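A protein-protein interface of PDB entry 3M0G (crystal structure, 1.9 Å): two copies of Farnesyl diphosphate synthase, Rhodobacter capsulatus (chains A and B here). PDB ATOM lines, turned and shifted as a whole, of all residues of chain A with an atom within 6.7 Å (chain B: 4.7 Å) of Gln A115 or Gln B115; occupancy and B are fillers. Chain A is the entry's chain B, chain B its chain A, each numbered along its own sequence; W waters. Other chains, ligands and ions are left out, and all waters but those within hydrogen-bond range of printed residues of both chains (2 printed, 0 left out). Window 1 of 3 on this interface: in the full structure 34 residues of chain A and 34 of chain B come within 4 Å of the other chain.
The side-chain carboxylate of Asp B112 sits at hydrogen-bond distance from a ring nitrogen (ND1) of His A80.
NE2 of Gln A115 lies within hydrogen-bond range of O of Asp B112, 3.4 Å away.
The backbone carbonyl oxygen (O) of Asp A112 is in hydrogen-bond range of the side-chain amide nitrogen (NE2) of Gln B115.
The side-chain amide nitrogen (NE2) of Gln B115 sits close to the side-chain amide nitrogen (NE2) of Gln A115 (3.3 Å).
OG1 of Thr A116 is in hydrogen-bond range of OE1 of Gln B115.
The side-chain hydroxyl (OG1) of Thr B116 sits at hydrogen-bond distance from the side-chain amide oxygen (OE1) of Gln A115 (2.5 Å).
The side-chain carboxylate (OD1) of Asp A112 lies close to the side-chain carboxylate (OD1) of Asp B112 (3.3 Å).
The backbone carbonyl oxygen of Asp B112 lies within hydrogen-bond range of the side-chain hydroxyl of Thr B116 (3.2 Å).
The side-chain hydroxyl (OH) of Tyr A76 lies within hydrogen-bond range of the side-chain amide nitrogen (NE2) of Gln A115, 3.3 Å away.
The backbone carbonyl oxygen (O) of Asp A112 is in hydrogen-bond range of the side-chain hydroxyl (OG1) of Thr A116, at 3.0 Å.
The backbone carbonyl oxygen (O) of Leu A140 lies within hydrogen-bond range of the side-chain hydroxyl (OG) of Ser A144, 2.7 Å away.
The backbone carbonyl oxygen (O) of Ser A144 lies within hydrogen-bond range of the backbone NH (N) of Val A150 (3.3 Å).
The backbone carbonyl oxygen (O) of Gly A145 sits at hydrogen-bond distance from the backbone NH (N) of Val A150.
Among the printed residues, merely in contact across the chains: Tyr A76 with Asp B112 (3.6 Å), Asp A112 with Tyr B76 (3.4 Å), Phe A119 with Thr B116 (3.8 Å), Phe A119 with Phe B119 (3.6 Å), Ser A144 with Thr B116 (3.9 Å), Gly A145 with Thr B116 (3.7 Å) and Val A150 with Ala B113 (3.9 Å).
Gln A115 touches just these residues of chain B: Asp B112, Gln B115 and Thr B116.
Gln B115 touches three residues of chain A.
Printed residues of chain B within 4 Å of Val A150: Ala B113.
Of the printed residues of chain B, His A80 touches Asp B112.
The nearest residue of chain A that does not touch Gln B115 is Gly A111 (5.1 Å).
Of the 11 printed residues of chain B, 6 touch a printed residue of chain A.
Hydrophobic or aromatic side chains of chain B that line the printed part of chain A: Tyr B76, Ala B113 and Phe B119.
Of the 22 printed residues of chain A, 9 touch a printed residue of chain B.
Printed residues of chain A that touch a printed residue of chain B: Tyr A76, His A80, Asp A112, Gln A115, Thr A116, Phe A119, Ser A144, Gly A145 and Val A150.
Hydrophobic or aromatic side chains of chain A within 4 Å of the printed part of chain B: Tyr A76, His A80, Phe A119 and Val A150.
Tyr A76 touches Asp B112, and with the chains exchanged Asp A112 touches Tyr B76.
Asp A112 touches Gln B115, and with the chains exchanged Gln A115 touches Asp B112.
Phe A119 touches Thr B116, but with the chains exchanged Thr A116 does not touch Phe B119 (4.2 Å).
Phe B119 touches its own counterpart, Phe A119.
11 positions are printed for both chains.
Water W1 lies within hydrogen-bond range of the side-chain hydroxyl (OH) of Tyr B76, the side-chain hydroxyl (OG1) of Thr A116 and the side-chain amide oxygen (OE1) of Gln B115.
Water W2 lies within hydrogen-bond range of OH of Tyr A76 (2.5 Å), O of Ser A144 (2.7 Å), OG1 of Thr B116 (2.9 Å) and OE1 of Gln A115 (3.4 Å).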
ATOM      1  N   MET A  34      16.362  39.672  21.393  1.00  0.00           N
ATOM      2  CA  MET A  34      16.984  38.552  20.671  1.00  0.00           C
ATOM      3  C   MET A  34      17.020  38.861  19.177  1.00  0.00           C
ATOM      4  O   MET A  34      18.058  38.731  18.527  1.00  0.00           O
ATOM      5  CB  MET A  34      16.205  37.249  20.897  1.00  0.00           C
ATOM      6  CG  MET A  34      16.118  36.817  22.353  1.00  0.00           C
ATOM      7  SD  MET A  34      14.949  35.272  22.617  1.00  0.00           S
ATOM      8  CE  MET A  34      16.005  33.949  21.636  1.00  0.00           C
ATOM      9  N   ALA A  69      22.010  28.123  13.846  1.00  0.00           N
ATOM     10  CA  ALA A  69      22.481  27.802  15.196  1.00  0.00           C
ATOM     11  C   ALA A  69      23.789  28.508  15.532  1.00  0.00           C
ATOM     12  O   ALA A  69      23.929  29.047  16.650  1.00  0.00           O
ATOM     13  CB  ALA A  69      22.629  26.286  15.383  1.00  0.00           C
ATOM     14  N   ALA A  72      23.171  32.217  15.872  1.00  0.00           N
ATOM     15  CA  ALA A  72      22.526  32.378  17.176  1.00  0.00           C
ATOM     16  C   ALA A  72      23.529  32.325  18.323  1.00  0.00           C
ATOM     17  O   ALA A  72      23.484  33.154  19.229  1.00  0.00           O
ATOM     18  CB  ALA A  72      21.438  31.327  17.371  1.00  0.00           C
ATOM     19  N   LEU A  73      24.424  31.333  18.294  1.00  0.00           N
ATOM     20  CA  LEU A  73      25.404  31.156  19.352  1.00  0.00           C
ATOM     21  C   LEU A  73      26.351  32.376  19.348  1.00  0.00           C
ATOM     22  O   LEU A  73      26.687  32.913  20.409  1.00  0.00           O
ATOM     23  CB  LEU A  73      26.160  29.808  19.185  1.00  0.00           C
ATOM     24  CG  LEU A  73      26.882  29.088  20.354  1.00  0.00           C
ATOM     25  CD1 LEU A  73      27.938  29.966  20.986  1.00  0.00           C
ATOM     26  CD2 LEU A  73      25.906  28.564  21.446  1.00  0.00           C
ATOM     27  N   TYR A  76      24.574  35.559  20.839  1.00  0.00           N
ATOM     28  CA  TYR A  76      24.459  35.563  22.290  1.00  0.00           C
ATOM     29  C   TYR A  76      25.802  35.961  22.953  1.00  0.00           C
ATOM     30  O   TYR A  76      25.824  36.673  23.976  1.00  0.00           O
ATOM     31  CB  TYR A  76      23.930  34.186  22.789  1.00  0.00           C
ATOM     32  CG  TYR A  76      24.912  33.413  23.605  1.00  0.00           C
ATOM     33  CD1 TYR A  76      25.531  32.264  23.106  1.00  0.00           C
ATOM     34  CD2 TYR A  76      25.201  33.805  24.893  1.00  0.00           C
ATOM     35  CE1 TYR A  76      26.447  31.558  23.866  1.00  0.00           C
ATOM     36  CE2 TYR A  76      26.128  33.121  25.668  1.00  0.00           C
ATOM     37  CZ  TYR A  76      26.734  32.001  25.159  1.00  0.00           C
ATOM     38  OH  TYR A  76      27.640  31.330  25.930  1.00  0.00           O
ATOM     39  N   HIS A  80      26.344  39.287  25.622  1.00  0.00           N
ATOM     40  CA  HIS A  80      26.975  39.299  26.942  1.00  0.00           C
ATOM     41  C   HIS A  80      28.311  40.049  26.981  1.00  0.00           C
ATOM     42  O   HIS A  80      28.620  40.710  27.968  1.00  0.00           O
ATOM     43  CB  HIS A  80      27.152  37.859  27.470  1.00  0.00           C
ATOM     44  CG  HIS A  80      25.869  37.186  27.848  1.00  0.00           C
ATOM     45  ND1 HIS A  80      25.813  35.874  28.272  1.00  0.00           N
ATOM     46  CD2 HIS A  80      24.592  37.647  27.879  1.00  0.00           C
ATOM     47  CE1 HIS A  80      24.556  35.555  28.538  1.00  0.00           C
ATOM     48  NE2 HIS A  80      23.794  36.610  28.306  1.00  0.00           N
ATOM     49  N   ALA A 110      18.508  37.753  27.088  1.00  0.00           N
ATOM     50  CA  ALA A 110      18.441  37.579  25.634  1.00  0.00           C
ATOM     51  C   ALA A 110      19.598  36.703  25.134  1.00  0.00           C
ATOM     52  O   ALA A 110      19.420  35.854  24.247  1.00  0.00           O
ATOM     53  CB  ALA A 110      18.385  38.930  24.929  1.00  0.00           C
ATOM     54  N   GLY A 111      20.780  36.906  25.693  1.00  0.00           N
ATOM     55  CA  GLY A 111      21.909  35.998  25.393  1.00  0.00           C
ATOM     56  C   GLY A 111      21.657  34.573  25.888  1.00  0.00           C
ATOM     57  O   GLY A 111      22.017  33.618  25.222  1.00  0.00           O
ATOM     58  N   ASP A 112      21.060  34.432  27.066  1.00  0.00           N
ATOM     59  CA  ASP A 112      20.733  33.111  27.600  1.00  0.00           C
ATOM     60  C   ASP A 112      19.807  32.354  26.632  1.00  0.00           C
ATOM     61  O   ASP A 112      20.031  31.173  26.331  1.00  0.00           O
ATOM     62  CB  ASP A 112      20.127  33.193  29.001  1.00  0.00           C
ATOM     63  CG  ASP A 112      21.155  33.517  30.086  1.00  0.00           C
ATOM     64  OD1 ASP A 112      22.398  33.479  29.863  1.00  0.00           O
ATOM     65  OD2 ASP A 112      20.703  33.813  31.198  1.00  0.00           O
ATOM     66  N   ALA A 113      18.792  33.044  26.108  1.00  0.00           N
ATOM     67  CA  ALA A 113      17.810  32.394  25.240  1.00  0.00           C
ATOM     68  C   ALA A 113      18.332  32.229  23.824  1.00  0.00           C
ATOM     69  O   ALA A 113      17.877  31.357  23.071  1.00  0.00           O
ATOM     70  CB  ALA A 113      16.481  33.164  25.266  1.00  0.00           C
ATOM     71  N   LEU A 114      19.299  33.064  23.433  1.00  0.00           N
ATOM     72  CA  LEU A 114      19.895  32.878  22.135  1.00  0.00           C
ATOM     73  C   LEU A 114      20.785  31.636  22.131  1.00  0.00           C
ATOM     74  O   LEU A 114      20.876  30.957  21.123  1.00  0.00           O
ATOM     75  CB  LEU A 114      20.663  34.113  21.678  1.00  0.00           C
ATOM     76  CG  LEU A 114      19.764  35.204  21.083  1.00  0.00           C
ATOM     77  CD1 LEU A 114      20.521  36.530  21.130  1.00  0.00           C
ATOM     78  CD2 LEU A 114      19.354  34.846  19.659  1.00  0.00           C
ATOM     79  N   GLN A 115      21.423  31.335  23.264  1.00  0.00           N
ATOM     80  CA  GLN A 115      22.222  30.087  23.350  1.00  0.00           C
ATOM     81  C   GLN A 115      21.314  28.857  23.340  1.00  0.00           C
ATOM     82  O   GLN A 115      21.633  27.839  22.700  1.00  0.00           O
ATOM     83  CB  GLN A 115      23.152  30.066  24.573  1.00  0.00           C
ATOM     84  CG  GLN A 115      23.716  28.641  24.802  1.00  0.00           C
ATOM     85  CD  GLN A 115      24.823  28.538  25.829  1.00  0.00           C
ATOM     86  OE1 GLN A 115      25.533  27.518  25.882  1.00  0.00           O
ATOM     87  NE2 GLN A 115      24.986  29.575  26.639  1.00  0.00           N
ATOM     88  N   THR A 116      20.172  28.973  24.013  1.00  0.00           N
ATOM     89  CA  THR A 116      19.148  27.933  24.011  1.00  0.00           C
ATOM     90  C   THR A 116      18.567  27.758  22.611  1.00  0.00           C
ATOM     91  O   THR A 116      18.339  26.640  22.162  1.00  0.00           O
ATOM     92  CB  THR A 116      17.979  28.269  24.999  1.00  0.00           C
ATOM     93  OG1 THR A 116      18.509  28.574  26.290  1.00  0.00           O
ATOM     94  CG2 THR A 116      17.060  27.070  25.134  1.00  0.00           C
ATOM     95  N   LEU A 117      18.324  28.871  21.924  1.00  0.00           N
ATOM     96  CA  LEU A 117      17.842  28.819  20.540  1.00  0.00           C
ATOM     97  C   LEU A 117      18.807  28.077  19.608  1.00  0.00           C
ATOM     98  O   LEU A 117      18.352  27.260  18.767  1.00  0.00           O
ATOM     99  CB  LEU A 117      17.545  30.236  19.990  1.00  0.00           C
ATOM    100  CG  LEU A 117      16.800  30.319  18.646  1.00  0.00           C
ATOM    101  CD1 LEU A 117      15.393  29.704  18.752  1.00  0.00           C
ATOM    102  CD2 LEU A 117      16.670  31.773  18.210  1.00  0.00           C
ATOM    103  N   ALA A 118      20.102  28.397  19.708  1.00  0.00           N
ATOM    104  CA  ALA A 118      21.155  27.719  18.937  1.00  0.00           C
ATOM    105  C   ALA A 118      21.064  26.183  19.030  1.00  0.00           C
ATOM    106  O   ALA A 118      21.084  25.489  18.008  1.00  0.00           O
ATOM    107  CB  ALA A 118      22.557  28.178  19.365  1.00  0.00           C
ATOM    108  N   PHE A 119      20.972  25.670  20.245  1.00  0.00           N
ATOM    109  CA  PHE A 119      20.821  24.217  20.490  1.00  0.00           C
ATOM    110  C   PHE A 119      19.517  23.614  19.962  1.00  0.00           C
ATOM    111  O   PHE A 119      19.500  22.458  19.482  1.00  0.00           O
ATOM    112  CB  PHE A 119      21.098  23.876  21.970  1.00  0.00           C
ATOM    113  CG  PHE A 119      22.570  23.871  22.304  1.00  0.00           C
ATOM    114  CD1 PHE A 119      23.395  22.840  21.838  1.00  0.00           C
ATOM    115  CD2 PHE A 119      23.138  24.910  23.029  1.00  0.00           C
ATOM    116  CE1 PHE A 119      24.762  22.841  22.101  1.00  0.00           C
ATOM    117  CE2 PHE A 119      24.525  24.928  23.316  1.00  0.00           C
ATOM    118  CZ  PHE A 119      25.326  23.879  22.870  1.00  0.00           C
ATOM    119  N   GLU A 120      18.440  24.396  20.015  1.00  0.00           N
ATOM    120  CA  GLU A 120      17.125  23.931  19.583  1.00  0.00           C
ATOM    121  C   GLU A 120      17.183  23.733  18.074  1.00  0.00           C
ATOM    122  O   GLU A 120      16.718  22.732  17.534  1.00  0.00           O
ATOM    123  CB  GLU A 120      16.054  24.967  19.932  1.00  0.00           C
ATOM    124  CG  GLU A 120      14.632  24.562  19.519  1.00  0.00           C
ATOM    125  CD  GLU A 120      13.548  25.317  20.292  1.00  0.00           C
ATOM    126  OE1 GLU A 120      13.354  26.532  20.048  1.00  0.00           O
ATOM    127  OE2 GLU A 120      12.874  24.686  21.130  1.00  0.00           O
ATOM    128  N   LEU A 140      28.813  21.582  18.831  1.00  0.00           N
ATOM    129  CA  LEU A 140      28.469  22.963  19.203  1.00  0.00           C
ATOM    130  C   LEU A 140      28.776  23.196  20.659  1.00  0.00           C
ATOM    131  O   LEU A 140      29.337  24.235  21.029  1.00  0.00           O
ATOM    132  CB  LEU A 140      26.974  23.247  18.945  1.00  0.00           C
ATOM    133  CG  LEU A 140      26.448  24.674  19.186  1.00  0.00           C
ATOM    134  CD1 LEU A 140      27.278  25.747  18.449  1.00  0.00           C
ATOM    135  CD2 LEU A 140      24.954  24.842  18.912  1.00  0.00           C
ATOM    136  N   SER A 144      31.592  25.823  22.360  1.00  0.00           N
ATOM    137  CA  SER A 144      30.967  27.025  22.893  1.00  0.00           C
ATOM    138  C   SER A 144      31.190  27.137  24.383  1.00  0.00           C
ATOM    139  O   SER A 144      31.081  28.224  24.927  1.00  0.00           O
ATOM    140  CB  SER A 144      29.454  27.022  22.630  1.00  0.00           C
ATOM    141  OG  SER A 144      29.208  26.956  21.231  1.00  0.00           O
ATOM    142  N   GLY A 145      31.448  26.002  25.029  1.00  0.00           N
ATOM    143  CA  GLY A 145      31.464  25.952  26.498  1.00  0.00           C
ATOM    144  C   GLY A 145      32.811  26.230  27.081  1.00  0.00           C
ATOM    145  O   GLY A 145      33.662  26.868  26.438  1.00  0.00           O
ATOM    146  N   MET A 149      34.673  28.370  23.677  1.00  0.00           N
ATOM    147  CA  MET A 149      34.364  29.808  23.658  1.00  0.00           C
ATOM    148  C   MET A 149      34.377  30.531  24.986  1.00  0.00           C
ATOM    149  O   MET A 149      35.049  31.554  25.083  1.00  0.00           O
ATOM    150  CB  MET A 149      33.054  30.103  22.959  1.00  0.00           C
ATOM    151  CG  MET A 149      32.947  31.560  22.492  1.00  0.00           C
ATOM    152  SD  MET A 149      31.201  31.909  21.752  1.00  0.00           S
ATOM    153  CE  MET A 149      30.190  31.471  23.405  1.00  0.00           C
ATOM    154  N   VAL A 150      33.600  30.046  25.967  1.00  0.00           N
ATOM    155  CA  VAL A 150      33.524  30.705  27.301  1.00  0.00           C
ATOM    156  C   VAL A 150      34.868  30.665  28.013  1.00  0.00           C
ATOM    157  O   VAL A 150      35.212  31.576  28.797  1.00  0.00           O
ATOM    158  CB  VAL A 150      32.373  30.125  28.222  1.00  0.00           C
ATOM    159  CG1 VAL A 150      32.393  30.769  29.592  1.00  0.00           C
ATOM    160  CG2 VAL A 150      30.986  30.312  27.587  1.00  0.00           C
ATOM    161  N   LEU B  73      21.633  22.988  34.094  1.00  0.00           N
ATOM    162  CA  LEU B  73      20.735  24.024  33.615  1.00  0.00           C
ATOM    163  C   LEU B  73      20.156  24.841  34.780  1.00  0.00           C
ATOM    164  O   LEU B  73      20.156  26.074  34.725  1.00  0.00           O
ATOM    165  CB  LEU B  73      19.631  23.388  32.746  1.00  0.00           C
ATOM    166  CG  LEU B  73      18.858  24.204  31.698  1.00  0.00           C
ATOM    167  CD1 LEU B  73      18.093  25.294  32.403  1.00  0.00           C
ATOM    168  CD2 LEU B  73      19.719  24.769  30.547  1.00  0.00           C
ATOM    169  N   TYR B  76      22.920  27.080  36.404  1.00  0.00           N
ATOM    170  CA  TYR B  76      23.198  28.247  35.575  1.00  0.00           C
ATOM    171  C   TYR B  76      22.127  29.319  35.779  1.00  0.00           C
ATOM    172  O   TYR B  76      22.435  30.518  35.761  1.00  0.00           O
ATOM    173  CB  TYR B  76      23.321  27.859  34.075  1.00  0.00           C
ATOM    174  CG  TYR B  76      22.321  28.490  33.139  1.00  0.00           C
ATOM    175  CD1 TYR B  76      21.353  27.716  32.496  1.00  0.00           C
ATOM    176  CD2 TYR B  76      22.382  29.852  32.841  1.00  0.00           C
ATOM    177  CE1 TYR B  76      20.447  28.276  31.649  1.00  0.00           C
ATOM    178  CE2 TYR B  76      21.464  30.433  31.984  1.00  0.00           C
ATOM    179  CZ  TYR B  76      20.503  29.643  31.391  1.00  0.00           C
ATOM    180  OH  TYR B  76      19.591  30.212  30.528  1.00  0.00           O
ATOM    181  N   GLY B 111      27.620  30.820  34.249  1.00  0.00           N
ATOM    182  CA  GLY B 111      26.237  30.453  33.985  1.00  0.00           C
ATOM    183  C   GLY B 111      26.153  30.062  32.520  1.00  0.00           C
ATOM    184  O   GLY B 111      25.555  29.048  32.173  1.00  0.00           O
ATOM    185  N   ASP B 112      26.800  30.869  31.688  1.00  0.00           N
ATOM    186  CA  ASP B 112      26.878  30.614  30.254  1.00  0.00           C
ATOM    187  C   ASP B 112      27.446  29.215  29.997  1.00  0.00           C
ATOM    188  O   ASP B 112      26.822  28.422  29.318  1.00  0.00           O
ATOM    189  CB  ASP B 112      27.716  31.713  29.583  1.00  0.00           C
ATOM    190  CG  ASP B 112      26.899  32.994  29.292  1.00  0.00           C
ATOM    191  OD1 ASP B 112      25.660  33.031  29.540  1.00  0.00           O
ATOM    192  OD2 ASP B 112      27.515  33.981  28.839  1.00  0.00           O
ATOM    193  N   ALA B 113      28.593  28.881  30.588  1.00  0.00           N
ATOM    194  CA  ALA B 113      29.184  27.548  30.366  1.00  0.00           C
ATOM    195  C   ALA B 113      28.408  26.403  31.012  1.00  0.00           C
ATOM    196  O   ALA B 113      28.506  25.282  30.552  1.00  0.00           O
ATOM    197  CB  ALA B 113      30.628  27.507  30.807  1.00  0.00           C
ATOM    198  N   LEU B 114      27.671  26.681  32.078  1.00  0.00           N
ATOM    199  CA  LEU B 114      26.831  25.665  32.703  1.00  0.00           C
ATOM    200  C   LEU B 114      25.663  25.257  31.814  1.00  0.00           C
ATOM    201  O   LEU B 114      25.281  24.085  31.794  1.00  0.00           O
ATOM    202  CB  LEU B 114      26.317  26.124  34.060  1.00  0.00           C
ATOM    203  CG  LEU B 114      27.235  25.808  35.247  1.00  0.00           C
ATOM    204  CD1 LEU B 114      26.797  26.664  36.435  1.00  0.00           C
ATOM    205  CD2 LEU B 114      27.194  24.334  35.597  1.00  0.00           C
ATOM    206  N   GLN B 115      25.104  26.226  31.089  1.00  0.00           N
ATOM    207  CA  GLN B 115      24.080  25.928  30.090  1.00  0.00           C
ATOM    208  C   GLN B 115      24.627  25.075  28.950  1.00  0.00           C
ATOM    209  O   GLN B 115      23.970  24.116  28.524  1.00  0.00           O
ATOM    210  CB  GLN B 115      23.408  27.201  29.543  1.00  0.00           C
ATOM    211  CG  GLN B 115      22.585  26.943  28.238  1.00  0.00           C
ATOM    212  CD  GLN B 115      21.546  28.022  27.916  1.00  0.00           C
ATOM    213  OE1 GLN B 115      20.404  27.702  27.625  1.00  0.00           O
ATOM    214  NE2 GLN B 115      21.938  29.279  27.940  1.00  0.00           N
ATOM    215  N   THR B 116      25.824  25.416  28.462  1.00  0.00           N
ATOM    216  CA  THR B 116      26.440  24.625  27.403  1.00  0.00           C
ATOM    217  C   THR B 116      26.710  23.202  27.868  1.00  0.00           C
ATOM    218  O   THR B 116      26.525  22.269  27.117  1.00  0.00           O
ATOM    219  CB  THR B 116      27.763  25.218  26.888  1.00  0.00           C
ATOM    220  OG1 THR B 116      27.681  26.639  26.860  1.00  0.00           O
ATOM    221  CG2 THR B 116      28.004  24.736  25.495  1.00  0.00           C
ATOM    222  N   LEU B 117      27.162  23.051  29.115  1.00  0.00           N
ATOM    223  CA  LEU B 117      27.386  21.732  29.697  1.00  0.00           C
ATOM    224  C   LEU B 117      26.098  20.902  29.785  1.00  0.00           C
ATOM    225  O   LEU B 117      26.116  19.685  29.596  1.00  0.00           O
ATOM    226  CB  LEU B 117      28.055  21.841  31.080  1.00  0.00           C
ATOM    227  CG  LEU B 117      28.364  20.461  31.721  1.00  0.00           C
ATOM    228  CD1 LEU B 117      29.277  19.581  30.866  1.00  0.00           C
ATOM    229  CD2 LEU B 117      28.929  20.616  33.110  1.00  0.00           C
ATOM    230  N   ALA B 118      24.967  21.548  30.059  1.00  0.00           N
ATOM    231  CA  ALA B 118      23.724  20.801  30.140  1.00  0.00           C
ATOM    232  C   ALA B 118      23.392  20.172  28.782  1.00  0.00           C
ATOM    233  O   ALA B 118      22.971  18.999  28.716  1.00  0.00           O
ATOM    234  CB  ALA B 118      22.576  21.674  30.660  1.00  0.00           C
ATOM    235  N   PHE B 119      23.634  20.927  27.717  1.00  0.00           N
ATOM    236  CA  PHE B 119      23.377  20.447  26.336  1.00  0.00           C
ATOM    237  C   PHE B 119      24.380  19.356  25.911  1.00  0.00           C
ATOM    238  O   PHE B 119      23.979  18.341  25.321  1.00  0.00           O
ATOM    239  CB  PHE B 119      23.233  21.624  25.359  1.00  0.00           C
ATOM    240  CG  PHE B 119      21.897  22.348  25.499  1.00  0.00           C
ATOM    241  CD1 PHE B 119      20.741  21.807  24.931  1.00  0.00           C
ATOM    242  CD2 PHE B 119      21.784  23.517  26.260  1.00  0.00           C
ATOM    243  CE1 PHE B 119      19.483  22.435  25.089  1.00  0.00           C
ATOM    244  CE2 PHE B 119      20.538  24.157  26.429  1.00  0.00           C
ATOM    245  CZ  PHE B 119      19.386  23.612  25.847  1.00  0.00           C
HETATM  246  O   HOH W   1      18.075  28.885  29.031  1.00  0.00           O
HETATM  247  O   HOH W   2      28.520  29.003  25.386  1.00  0.00           O
